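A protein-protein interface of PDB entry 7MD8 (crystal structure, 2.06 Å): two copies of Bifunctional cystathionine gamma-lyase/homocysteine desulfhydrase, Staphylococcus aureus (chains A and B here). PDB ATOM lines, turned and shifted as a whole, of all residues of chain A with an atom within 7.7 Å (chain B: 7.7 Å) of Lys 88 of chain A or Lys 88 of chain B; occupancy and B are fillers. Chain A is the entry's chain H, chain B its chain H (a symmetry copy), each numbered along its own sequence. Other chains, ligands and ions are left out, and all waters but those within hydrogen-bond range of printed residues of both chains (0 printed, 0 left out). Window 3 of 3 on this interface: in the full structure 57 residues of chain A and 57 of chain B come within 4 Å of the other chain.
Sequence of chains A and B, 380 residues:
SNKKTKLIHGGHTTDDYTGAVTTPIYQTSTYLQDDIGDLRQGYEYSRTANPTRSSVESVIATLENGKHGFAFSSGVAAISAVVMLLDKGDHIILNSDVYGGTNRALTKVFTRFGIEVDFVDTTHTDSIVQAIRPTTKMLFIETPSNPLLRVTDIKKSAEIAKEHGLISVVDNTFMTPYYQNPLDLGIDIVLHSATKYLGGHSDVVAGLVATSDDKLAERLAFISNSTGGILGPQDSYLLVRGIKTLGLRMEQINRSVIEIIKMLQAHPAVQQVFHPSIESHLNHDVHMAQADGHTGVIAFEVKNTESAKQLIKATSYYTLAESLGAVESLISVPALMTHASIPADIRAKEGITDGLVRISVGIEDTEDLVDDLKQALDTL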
ATOM      1  N   LEU A  86      16.503  16.788 -17.511  1.00  0.00           N
ATOM      2  CA  LEU A  86      16.889  17.004 -18.899  1.00  0.00           C
ATOM      3  C   LEU A  86      16.915  15.688 -19.673  1.00  0.00           C
ATOM      4  O   LEU A  86      16.860  14.593 -19.103  1.00  0.00           O
ATOM      5  CB  LEU A  86      18.256  17.685 -18.983  1.00  0.00           C
ATOM      6  CG  LEU A  86      18.357  19.007 -18.219  1.00  0.00           C
ATOM      7  CD1 LEU A  86      19.699  19.693 -18.422  1.00  0.00           C
ATOM      8  CD2 LEU A  86      17.217  19.927 -18.598  1.00  0.00           C
ATOM      9  N   ASP A  87      17.005  15.812 -20.997  1.00  0.00           N
ATOM     10  CA  ASP A  87      17.115  14.691 -21.919  1.00  0.00           C
ATOM     11  C   ASP A  87      18.446  14.744 -22.642  1.00  0.00           C
ATOM     12  O   ASP A  87      19.106  15.784 -22.703  1.00  0.00           O
ATOM     13  CB  ASP A  87      16.021  14.709 -22.996  1.00  0.00           C
ATOM     14  CG  ASP A  87      14.628  14.547 -22.437  1.00  0.00           C
ATOM     15  OD1 ASP A  87      14.470  14.109 -21.271  1.00  0.00           O
ATOM     16  OD2 ASP A  87      13.680  14.882 -23.174  1.00  0.00           O
ATOM     17  N   LYS A  88      18.804  13.608 -23.229  1.00  0.00           N
ATOM     18  CA  LYS A  88      19.890  13.527 -24.194  1.00  0.00           C
ATOM     19  C   LYS A  88      19.773  14.647 -25.227  1.00  0.00           C
ATOM     20  O   LYS A  88      18.689  14.915 -25.747  1.00  0.00           O
ATOM     21  CB  LYS A  88      19.837  12.157 -24.872  1.00  0.00           C
ATOM     22  CG  LYS A  88      20.625  12.030 -26.145  1.00  0.00           C
ATOM     23  CD  LYS A  88      20.297  10.709 -26.834  1.00  0.00           C
ATOM     24  N   GLY A  89      20.889  15.332 -25.484  1.00  0.00           N
ATOM     25  CA  GLY A  89      20.907  16.487 -26.359  1.00  0.00           C
ATOM     26  C   GLY A  89      20.686  17.824 -25.675  1.00  0.00           C
ATOM     27  O   GLY A  89      20.951  18.867 -26.285  1.00  0.00           O
ATOM     28  N   ASP A  90      20.210  17.831 -24.431  1.00  0.00           N
ATOM     29  CA  ASP A  90      20.044  19.084 -23.712  1.00  0.00           C
ATOM     30  C   ASP A  90      21.386  19.594 -23.191  1.00  0.00           C
ATOM     31  O   ASP A  90      22.336  18.839 -22.969  1.00  0.00           O
ATOM     32  CB  ASP A  90      19.079  18.930 -22.538  1.00  0.00           C
ATOM     33  CG  ASP A  90      17.645  18.752 -22.972  1.00  0.00           C
ATOM     34  OD1 ASP A  90      17.346  18.957 -24.173  1.00  0.00           O
ATOM     35  OD2 ASP A  90      16.814  18.410 -22.098  1.00  0.00           O
ATOM     36  N   HIS A  91      21.434  20.897 -22.963  1.00  0.00           N
ATOM     37  CA  HIS A  91      22.651  21.588 -22.573  1.00  0.00           C
ATOM     38  C   HIS A  91      22.414  22.295 -21.246  1.00  0.00           C
ATOM     39  O   HIS A  91      21.337  22.855 -21.014  1.00  0.00           O
ATOM     40  CB  HIS A  91      23.056  22.577 -23.686  1.00  0.00           C
ATOM     41  CG  HIS A  91      24.262  23.409 -23.377  1.00  0.00           C
ATOM     42  ND1 HIS A  91      24.192  24.776 -23.189  1.00  0.00           N
ATOM     43  CD2 HIS A  91      25.575  23.083 -23.287  1.00  0.00           C
ATOM     44  CE1 HIS A  91      25.406  25.252 -22.964  1.00  0.00           C
ATOM     45  NE2 HIS A  91      26.264  24.245 -23.016  1.00  0.00           N
ATOM     46  N   VAL A 109      29.510  11.326 -15.673  1.00  0.00           N
ATOM     47  CA  VAL A 109      28.313  10.493 -15.703  1.00  0.00           C
ATOM     48  C   VAL A 109      27.322  10.999 -16.746  1.00  0.00           C
ATOM     49  O   VAL A 109      27.052  10.321 -17.737  1.00  0.00           O
ATOM     50  CB  VAL A 109      27.662  10.387 -14.304  1.00  0.00           C
ATOM     51  CG1 VAL A 109      26.363   9.601 -14.382  1.00  0.00           C
ATOM     52  CG2 VAL A 109      28.628   9.732 -13.315  1.00  0.00           C
ATOM     53  N   PHE A 110      26.803  12.209 -16.565  1.00  0.00           N
ATOM     54  CA  PHE A 110      25.700  12.620 -17.421  1.00  0.00           C
ATOM     55  C   PHE A 110      26.117  12.936 -18.856  1.00  0.00           C
ATOM     56  O   PHE A 110      25.271  12.839 -19.752  1.00  0.00           O
ATOM     57  CB  PHE A 110      24.968  13.787 -16.773  1.00  0.00           C
ATOM     58  CG  PHE A 110      24.194  13.366 -15.561  1.00  0.00           C
ATOM     59  CD1 PHE A 110      23.020  12.628 -15.701  1.00  0.00           C
ATOM     60  CD2 PHE A 110      24.678  13.623 -14.283  1.00  0.00           C
ATOM     61  CE1 PHE A 110      22.318  12.197 -14.591  1.00  0.00           C
ATOM     62  CE2 PHE A 110      23.975  13.190 -13.158  1.00  0.00           C
ATOM     63  CZ  PHE A 110      22.798  12.480 -13.314  1.00  0.00           C
ATOM     64  N   THR A 111      27.388  13.266 -19.121  1.00  0.00           N
ATOM     65  CA  THR A 111      27.770  13.438 -20.526  1.00  0.00           C
ATOM     66  C   THR A 111      27.698  12.118 -21.281  1.00  0.00           C
ATOM     67  O   THR A 111      27.456  12.114 -22.494  1.00  0.00           O
ATOM     68  CB  THR A 111      29.169  14.044 -20.677  1.00  0.00           C
ATOM     69  OG1 THR A 111      30.111  13.297 -19.899  1.00  0.00           O
ATOM     70  CG2 THR A 111      29.179  15.509 -20.243  1.00  0.00           C
ATOM     71  N   ARG A 112      27.886  10.992 -20.584  1.00  0.00           N
ATOM     72  CA  ARG A 112      27.700   9.693 -21.218  1.00  0.00           C
ATOM     73  C   ARG A 112      26.251   9.464 -21.617  1.00  0.00           C
ATOM     74  O   ARG A 112      25.979   8.601 -22.460  1.00  0.00           O
ATOM     75  CB  ARG A 112      28.174   8.574 -20.291  1.00  0.00           C
ATOM     76  CG  ARG A 112      29.656   8.641 -19.946  1.00  0.00           C
ATOM     77  CD  ARG A 112      30.122   7.384 -19.227  1.00  0.00           C
ATOM     78  NE  ARG A 112      29.603   7.296 -17.864  1.00  0.00           N
ATOM     79  CZ  ARG A 112      28.607   6.497 -17.482  1.00  0.00           C
ATOM     80  NH1 ARG A 112      28.003   5.703 -18.357  1.00  0.00           N
ATOM     81  NH2 ARG A 112      28.211   6.496 -16.212  1.00  0.00           N
ATOM     82  N   PHE A 113      25.321  10.227 -21.046  1.00  0.00           N
ATOM     83  CA  PHE A 113      23.918  10.184 -21.430  1.00  0.00           C
ATOM     84  C   PHE A 113      23.537  11.337 -22.346  1.00  0.00           C
ATOM     85  O   PHE A 113      22.347  11.654 -22.476  1.00  0.00           O
ATOM     86  CB  PHE A 113      23.038  10.171 -20.183  1.00  0.00           C
ATOM     87  CG  PHE A 113      23.412   9.088 -19.219  1.00  0.00           C
ATOM     88  CD1 PHE A 113      23.685   7.814 -19.679  1.00  0.00           C
ATOM     89  CD2 PHE A 113      23.528   9.346 -17.872  1.00  0.00           C
ATOM     90  CE1 PHE A 113      24.054   6.811 -18.820  1.00  0.00           C
ATOM     91  CE2 PHE A 113      23.901   8.342 -17.002  1.00  0.00           C
ATOM     92  CZ  PHE A 113      24.171   7.069 -17.487  1.00  0.00           C
ATOM     93  N   GLY A 114      24.521  11.971 -22.979  1.00  0.00           N
ATOM     94  CA  GLY A 114      24.223  12.990 -23.964  1.00  0.00           C
ATOM     95  C   GLY A 114      23.799  14.331 -23.412  1.00  0.00           C
ATOM     96  O   GLY A 114      23.322  15.166 -24.183  1.00  0.00           O
ATOM     97  N   ILE A 115      23.930  14.562 -22.108  1.00  0.00           N
ATOM     98  CA  ILE A 115      23.787  15.907 -21.560  1.00  0.00           C
ATOM     99  C   ILE A 115      25.058  16.682 -21.864  1.00  0.00           C
ATOM    100  O   ILE A 115      26.164  16.198 -21.599  1.00  0.00           O
ATOM    101  CB  ILE A 115      23.532  15.869 -20.045  1.00  0.00           C
ATOM    102  CG1 ILE A 115      22.377  14.925 -19.708  1.00  0.00           C
ATOM    103  CG2 ILE A 115      23.245  17.278 -19.521  1.00  0.00           C
ATOM    104  CD1 ILE A 115      21.063  15.406 -20.247  1.00  0.00           C
ATOM    105  N   GLU A 116      24.911  17.886 -22.405  1.00  0.00           N
ATOM    106  CA  GLU A 116      26.055  18.741 -22.698  1.00  0.00           C
ATOM    107  C   GLU A 116      26.195  19.820 -21.635  1.00  0.00           C
ATOM    108  O   GLU A 116      25.197  20.367 -21.151  1.00  0.00           O
ATOM    109  CB  GLU A 116      25.921  19.389 -24.074  1.00  0.00           C
ATOM    110  CG  GLU A 116      25.597  18.410 -25.166  1.00  0.00           C
ATOM    111  CD  GLU A 116      26.827  17.705 -25.696  1.00  0.00           C
ATOM    112  OE1 GLU A 116      27.801  17.511 -24.926  1.00  0.00           O
ATOM    113  OE2 GLU A 116      26.810  17.348 -26.892  1.00  0.00           O
ATOM    114  N   THR A 135      20.100  24.564 -27.703  1.00  0.00           N
ATOM    115  CA  THR A 135      19.782  23.370 -26.931  1.00  0.00           C
ATOM    116  C   THR A 135      19.869  23.569 -25.417  1.00  0.00           C
ATOM    117  O   THR A 135      19.681  22.601 -24.675  1.00  0.00           O
ATOM    118  CB  THR A 135      20.717  22.219 -27.318  1.00  0.00           C
ATOM    119  OG1 THR A 135      22.076  22.649 -27.162  1.00  0.00           O
ATOM    120  CG2 THR A 135      20.467  21.750 -28.760  1.00  0.00           C
ATOM    121  N   LEU B  86      25.954   1.773 -18.538  1.00  0.00           N
ATOM    122  CA  LEU B  86      25.826   1.914 -19.983  1.00  0.00           C
ATOM    123  C   LEU B  86      25.909   3.381 -20.401  1.00  0.00           C
ATOM    124  O   LEU B  86      25.837   4.300 -19.579  1.00  0.00           O
ATOM    125  CB  LEU B  86      24.511   1.305 -20.473  1.00  0.00           C
ATOM    126  CG  LEU B  86      24.306  -0.162 -20.088  1.00  0.00           C
ATOM    127  CD1 LEU B  86      23.037  -0.746 -20.690  1.00  0.00           C
ATOM    128  CD2 LEU B  86      25.515  -0.986 -20.472  1.00  0.00           C
ATOM    129  N   ASP B  87      26.059   3.588 -21.709  1.00  0.00           N
ATOM    130  CA  ASP B  87      26.090   4.903 -22.331  1.00  0.00           C
ATOM    131  C   ASP B  87      24.910   5.059 -23.271  1.00  0.00           C
ATOM    132  O   ASP B  87      24.295   4.081 -23.703  1.00  0.00           O
ATOM    133  CB  ASP B  87      27.359   5.125 -23.167  1.00  0.00           C
ATOM    134  CG  ASP B  87      28.625   5.113 -22.347  1.00  0.00           C
ATOM    135  OD1 ASP B  87      28.564   5.248 -21.100  1.00  0.00           O
ATOM    136  OD2 ASP B  87      29.698   4.949 -22.963  1.00  0.00           O
ATOM    137  N   LYS B  88      24.638   6.312 -23.615  1.00  0.00           N
ATOM    138  CA  LYS B  88      23.740   6.652 -24.708  1.00  0.00           C
ATOM    139  C   LYS B  88      24.063   5.818 -25.946  1.00  0.00           C
ATOM    140  O   LYS B  88      25.228   5.662 -26.315  1.00  0.00           O
ATOM    141  CB  LYS B  88      23.882   8.145 -25.008  1.00  0.00           C
ATOM    142  CG  LYS B  88      23.330   8.599 -26.330  1.00  0.00           C
ATOM    143  CD  LYS B  88      23.746  10.041 -26.604  1.00  0.00           C
ATOM    144  N   GLY B  89      23.026   5.242 -26.559  1.00  0.00           N
ATOM    145  CA  GLY B  89      23.191   4.338 -27.679  1.00  0.00           C
ATOM    146  C   GLY B  89      23.316   2.870 -27.317  1.00  0.00           C
ATOM    147  O   GLY B  89      23.188   2.014 -28.202  1.00  0.00           O
ATOM    148  N   ASP B  90      23.563   2.547 -26.048  1.00  0.00           N
ATOM    149  CA  ASP B  90      23.627   1.152 -25.642  1.00  0.00           C
ATOM    150  C   ASP B  90      22.225   0.560 -25.510  1.00  0.00           C
ATOM    151  O   ASP B  90      21.234   1.259 -25.282  1.00  0.00           O
ATOM    152  CB  ASP B  90      24.363   0.991 -24.313  1.00  0.00           C
ATOM    153  CG  ASP B  90      25.847   1.238 -24.428  1.00  0.00           C
ATOM    154  OD1 ASP B  90      26.360   1.327 -25.569  1.00  0.00           O
ATOM    155  OD2 ASP B  90      26.501   1.336 -23.363  1.00  0.00           O
ATOM    156  N   HIS B  91      22.166  -0.758 -25.621  1.00  0.00           N
ATOM    157  CA  HIS B  91      20.915  -1.496 -25.637  1.00  0.00           C
ATOM    158  C   HIS B  91      20.928  -2.513 -24.504  1.00  0.00           C
ATOM    159  O   HIS B  91      21.959  -3.137 -24.228  1.00  0.00           O
ATOM    160  CB  HIS B  91      20.737  -2.172 -27.012  1.00  0.00           C
ATOM    161  CG  HIS B  91      19.515  -3.027 -27.137  1.00  0.00           C
ATOM    162  ND1 HIS B  91      19.580  -4.400 -27.282  1.00  0.00           N
ATOM    163  CD2 HIS B  91      18.199  -2.704 -27.206  1.00  0.00           C
ATOM    164  CE1 HIS B  91      18.357  -4.889 -27.400  1.00  0.00           C
ATOM    165  NE2 HIS B  91      17.499  -3.881 -27.355  1.00  0.00           N
ATOM    166  N   VAL B 109      12.708   6.907 -17.763  1.00  0.00           N
ATOM    167  CA  VAL B 109      13.872   7.694 -17.373  1.00  0.00           C
ATOM    168  C   VAL B 109      15.044   7.439 -18.314  1.00  0.00           C
ATOM    169  O   VAL B 109      15.471   8.333 -19.044  1.00  0.00           O
ATOM    170  CB  VAL B 109      14.262   7.438 -15.898  1.00  0.00           C
ATOM    171  CG1 VAL B 109      15.535   8.191 -15.548  1.00  0.00           C
ATOM    172  CG2 VAL B 109      13.120   7.852 -14.967  1.00  0.00           C
ATOM    173  N   PHE B 110      15.549   6.210 -18.347  1.00  0.00           N
ATOM    174  CA  PHE B 110      16.796   5.997 -19.067  1.00  0.00           C
ATOM    175  C   PHE B 110      16.649   6.053 -20.586  1.00  0.00           C
ATOM    176  O   PHE B 110      17.639   6.348 -21.265  1.00  0.00           O
ATOM    177  CB  PHE B 110      17.427   4.690 -18.606  1.00  0.00           C
ATOM    178  CG  PHE B 110      17.964   4.783 -17.209  1.00  0.00           C
ATOM    179  CD1 PHE B 110      19.126   5.506 -16.952  1.00  0.00           C
ATOM    180  CD2 PHE B 110      17.266   4.230 -16.141  1.00  0.00           C
ATOM    181  CE1 PHE B 110      19.610   5.635 -15.663  1.00  0.00           C
ATOM    182  CE2 PHE B 110      17.747   4.358 -14.837  1.00  0.00           C
ATOM    183  CZ  PHE B 110      18.917   5.058 -14.602  1.00  0.00           C
ATOM    184  N   THR B 111      15.453   5.827 -21.147  1.00  0.00           N
ATOM    185  CA  THR B 111      15.332   6.013 -22.595  1.00  0.00           C
ATOM    186  C   THR B 111      15.508   7.477 -22.977  1.00  0.00           C
ATOM    187  O   THR B 111      15.961   7.774 -24.089  1.00  0.00           O
ATOM    188  CB  THR B 111      13.996   5.495 -23.138  1.00  0.00           C
ATOM    189  OG1 THR B 111      12.914   6.049 -22.380  1.00  0.00           O
ATOM    190  CG2 THR B 111      13.941   3.969 -23.086  1.00  0.00           C
ATOM    191  N   ARG B 112      15.173   8.401 -22.071  1.00  0.00           N
ATOM    192  CA  ARG B 112      15.441   9.811 -22.322  1.00  0.00           C
ATOM    193  C   ARG B 112      16.932  10.099 -22.388  1.00  0.00           C
ATOM    194  O   ARG B 112      17.330  11.136 -22.930  1.00  0.00           O
ATOM    195  CB  ARG B 112      14.783  10.679 -21.248  1.00  0.00           C
ATOM    196  CG  ARG B 112      13.266  10.562 -21.200  1.00  0.00           C
ATOM    197  CD  ARG B 112      12.651  11.614 -20.289  1.00  0.00           C
ATOM    198  NE  ARG B 112      12.917  11.352 -18.876  1.00  0.00           N
ATOM    199  CZ  ARG B 112      13.810  12.010 -18.138  1.00  0.00           C
ATOM    200  NH1 ARG B 112      14.543  12.981 -18.669  1.00  0.00           N
ATOM    201  NH2 ARG B 112      13.974  11.691 -16.858  1.00  0.00           N
ATOM    202  N   PHE B 113      17.762   9.198 -21.866  1.00  0.00           N
ATOM    203  CA  PHE B 113      19.210   9.303 -21.970  1.00  0.00           C
ATOM    204  C   PHE B 113      19.774   8.402 -23.058  1.00  0.00           C
ATOM    205  O   PHE B 113      20.974   8.100 -23.049  1.00  0.00           O
ATOM    206  CB  PHE B 113      19.853   8.989 -20.622  1.00  0.00           C
ATOM    207  CG  PHE B 113      19.289   9.810 -19.505  1.00  0.00           C
ATOM    208  CD1 PHE B 113      19.074  11.164 -19.678  1.00  0.00           C
ATOM    209  CD2 PHE B 113      18.940   9.231 -18.305  1.00  0.00           C
ATOM    210  CE1 PHE B 113      18.535  11.933 -18.679  1.00  0.00           C
ATOM    211  CE2 PHE B 113      18.396   9.999 -17.296  1.00  0.00           C
ATOM    212  CZ  PHE B 113      18.188  11.358 -17.493  1.00  0.00           C
ATOM    213  N   GLY B 114      18.932   7.965 -23.993  1.00  0.00           N
ATOM    214  CA  GLY B 114      19.424   7.213 -25.129  1.00  0.00           C
ATOM    215  C   GLY B 114      19.773   5.768 -24.857  1.00  0.00           C
ATOM    216  O   GLY B 114      20.398   5.138 -25.711  1.00  0.00           O
ATOM    217  N   ILE B 115      19.417   5.227 -23.695  1.00  0.00           N
ATOM    218  CA  ILE B 115      19.490   3.785 -23.478  1.00  0.00           C
ATOM    219  C   ILE B 115      18.311   3.138 -24.184  1.00  0.00           C
ATOM    220  O   ILE B 115      17.165   3.567 -24.009  1.00  0.00           O
ATOM    221  CB  ILE B 115      19.470   3.444 -21.979  1.00  0.00           C
ATOM    222  CG1 ILE B 115      20.525   4.251 -21.220  1.00  0.00           C
ATOM    223  CG2 ILE B 115      19.690   1.944 -21.775  1.00  0.00           C
ATOM    224  CD1 ILE B 115      21.924   3.887 -21.618  1.00  0.00           C
ATOM    225  N   GLU B 116      18.579   2.100 -24.969  1.00  0.00           N
ATOM    226  CA  GLU B 116      17.525   1.370 -25.662  1.00  0.00           C
ATOM    227  C   GLU B 116      17.222   0.066 -24.939  1.00  0.00           C
ATOM    228  O   GLU B 116      18.129  -0.605 -24.435  1.00  0.00           O
ATOM    229  CB  GLU B 116      17.916   1.077 -27.109  1.00  0.00           C
ATOM    230  CG  GLU B 116      18.407   2.287 -27.851  1.00  0.00           C
ATOM    231  CD  GLU B 116      17.277   3.127 -28.402  1.00  0.00           C
ATOM    232  OE1 GLU B 116      16.177   3.149 -27.794  1.00  0.00           O
ATOM    233  OE2 GLU B 116      17.499   3.768 -29.451  1.00  0.00           O
ATOM    234  N   THR B 135      24.406  -3.176 -30.801  1.00  0.00           N
ATOM    235  CA  THR B 135      24.554  -2.216 -29.716  1.00  0.00           C
ATOM    236  C   THR B 135      24.203  -2.780 -28.337  1.00  0.00           C
ATOM    237  O   THR B 135      24.234  -2.028 -27.359  1.00  0.00           O
ATOM    238  CB  THR B 135      23.677  -0.985 -29.968  1.00  0.00           C
ATOM    239  OG1 THR B 135      22.323  -1.409 -30.167  1.00  0.00           O
ATOM    240  CG2 THR B 135      24.170  -0.182 -31.182  1.00  0.00           C
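Of the 15 printed residues of chain B, 6 touch a printed residue of chain A. Hydrophobic or aromatic side chains of chain B that line the printed part of chain A: Phe 113. Among the printed residues, Asp or Glu carboxylates within 4 Å of a Lys or Arg side-chain nitrogen of the other chain: Asp 87 of chain A with Arg 112 of chain B and Arg 112 of chain A with Asp 87 of chain B.
The side-chain carboxylate of Asp 90 of chain A sits at hydrogen-bond distance from the backbone NH of Asp 87 of chain A (2.8 Å). O of Gly 114 of chain A sits at hydrogen-bond distance from N of Gly 89 of chain A, at 2.8 Å. The backbone NH (N) of Asp 87 of chain B sits at hydrogen-bond distance from the side-chain carboxylate (OD2) of Asp 90 of chain B, 2.8 Å away. The backbone carbonyl oxygen of Gly 114 of chain B lies within hydrogen-bond range of the backbone NH of Gly 89 of chain B (2.8 Å).
Leu 86 of chain A touches Phe 113 of chain B (O to CE1, 3.2 Å). Lys 88 of chain A touches Lys 88 of chain B (CD to CD, 3.5 Å). Gly 114 of chain B touches Lys 88 of chain A. Phe 113 of chain A touches Leu 86 of chain B (CE1 to O, 3.2 Å). Phe 113 of chain A touches Phe 113 of chain B (CB to CB, 3.4 Å). CA of Gly 114 of chain A touches CD of Lys 88 of chain B, 3.99 Å away.
Of the printed residues of chain B, Lys 88 of chain A touches Lys 88 (3.5 Å), Arg 112 (2.9 Å) and Gly 114 (3.99 Å). Of the printed residues of chain A, Lys 88 of chain B touches Lys 88, Arg 112 and Gly 114. Of the printed residues of chain B, Leu 86 of chain A touches Arg 112 and Phe 113. Printed residues of chain A within 4 Å of Gly 114 of chain B: Lys 88 (3.99 Å). Of the printed residues of chain A, Arg 112 of chain B touches Leu 86, Asp 87 and Lys 88. Of the printed residues of chain B, Phe 113 of chain A touches Leu 86 and Phe 113. Of the printed residues of chain A, Asp 87 of chain B touches Arg 112 (2.8 Å). The nearest printed residue of chain B that does not touch Lys 88 of chain A is Phe 113 of chain B (4.1 Å). The nearest printed residue of chain A that does not touch Gly 114 of chain B is Phe 113 of chain A (5.3 Å).
The backbone carbonyl oxygen (O) of Leu 86 of chain A is in hydrogen-bond range of the guanidinium group (NH1) of Arg 112 of chain B (2.9 Å). NH1 of Arg 112 of chain B is in salt-bridge range of OD1 of Asp 87 of chain A (2.8 Å). O of Arg 112 of chain B is in hydrogen-bond range of N of Lys 88 of chain A (2.9 Å). The guanidinium group (NH1) of Arg 112 of chain A lies within hydrogen-bond range of the backbone carbonyl oxygen (O) of Leu 86 of chain B, 2.9 Å away. NH1 of Arg 112 of chain A lies within salt-bridge range of OD1 of Asp 87 of chain B (2.8 Å). N of Lys 88 of chain B is in hydrogen-bond range of O of Arg 112 of chain A (2.9 Å).
Leu 86 of chain A touches Arg 112 of chain B, and with the chains exchanged Arg 112 of chain A touches Leu 86 of chain B. Leu 86 of chain A touches Phe 113 of chain B, and with the chains exchanged Phe 113 of chain A touches Leu 86 of chain B. Lys 88 of chain A touches Gly 114 of chain B, and with the chains exchanged Gly 114 of chain A touches Lys 88 of chain B. Phe 113 of chain B touches its own counterpart, Phe 113 of chain A. Positions printed for both chains: 86, 87, 88, 89, 90, 91, 109, 110, 111, 112, 113, 114, 115, 116 and 135. Of the 12 pairs that touch across the chains among the printed residues, 12 have their exchanged pair printed and touching as well.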
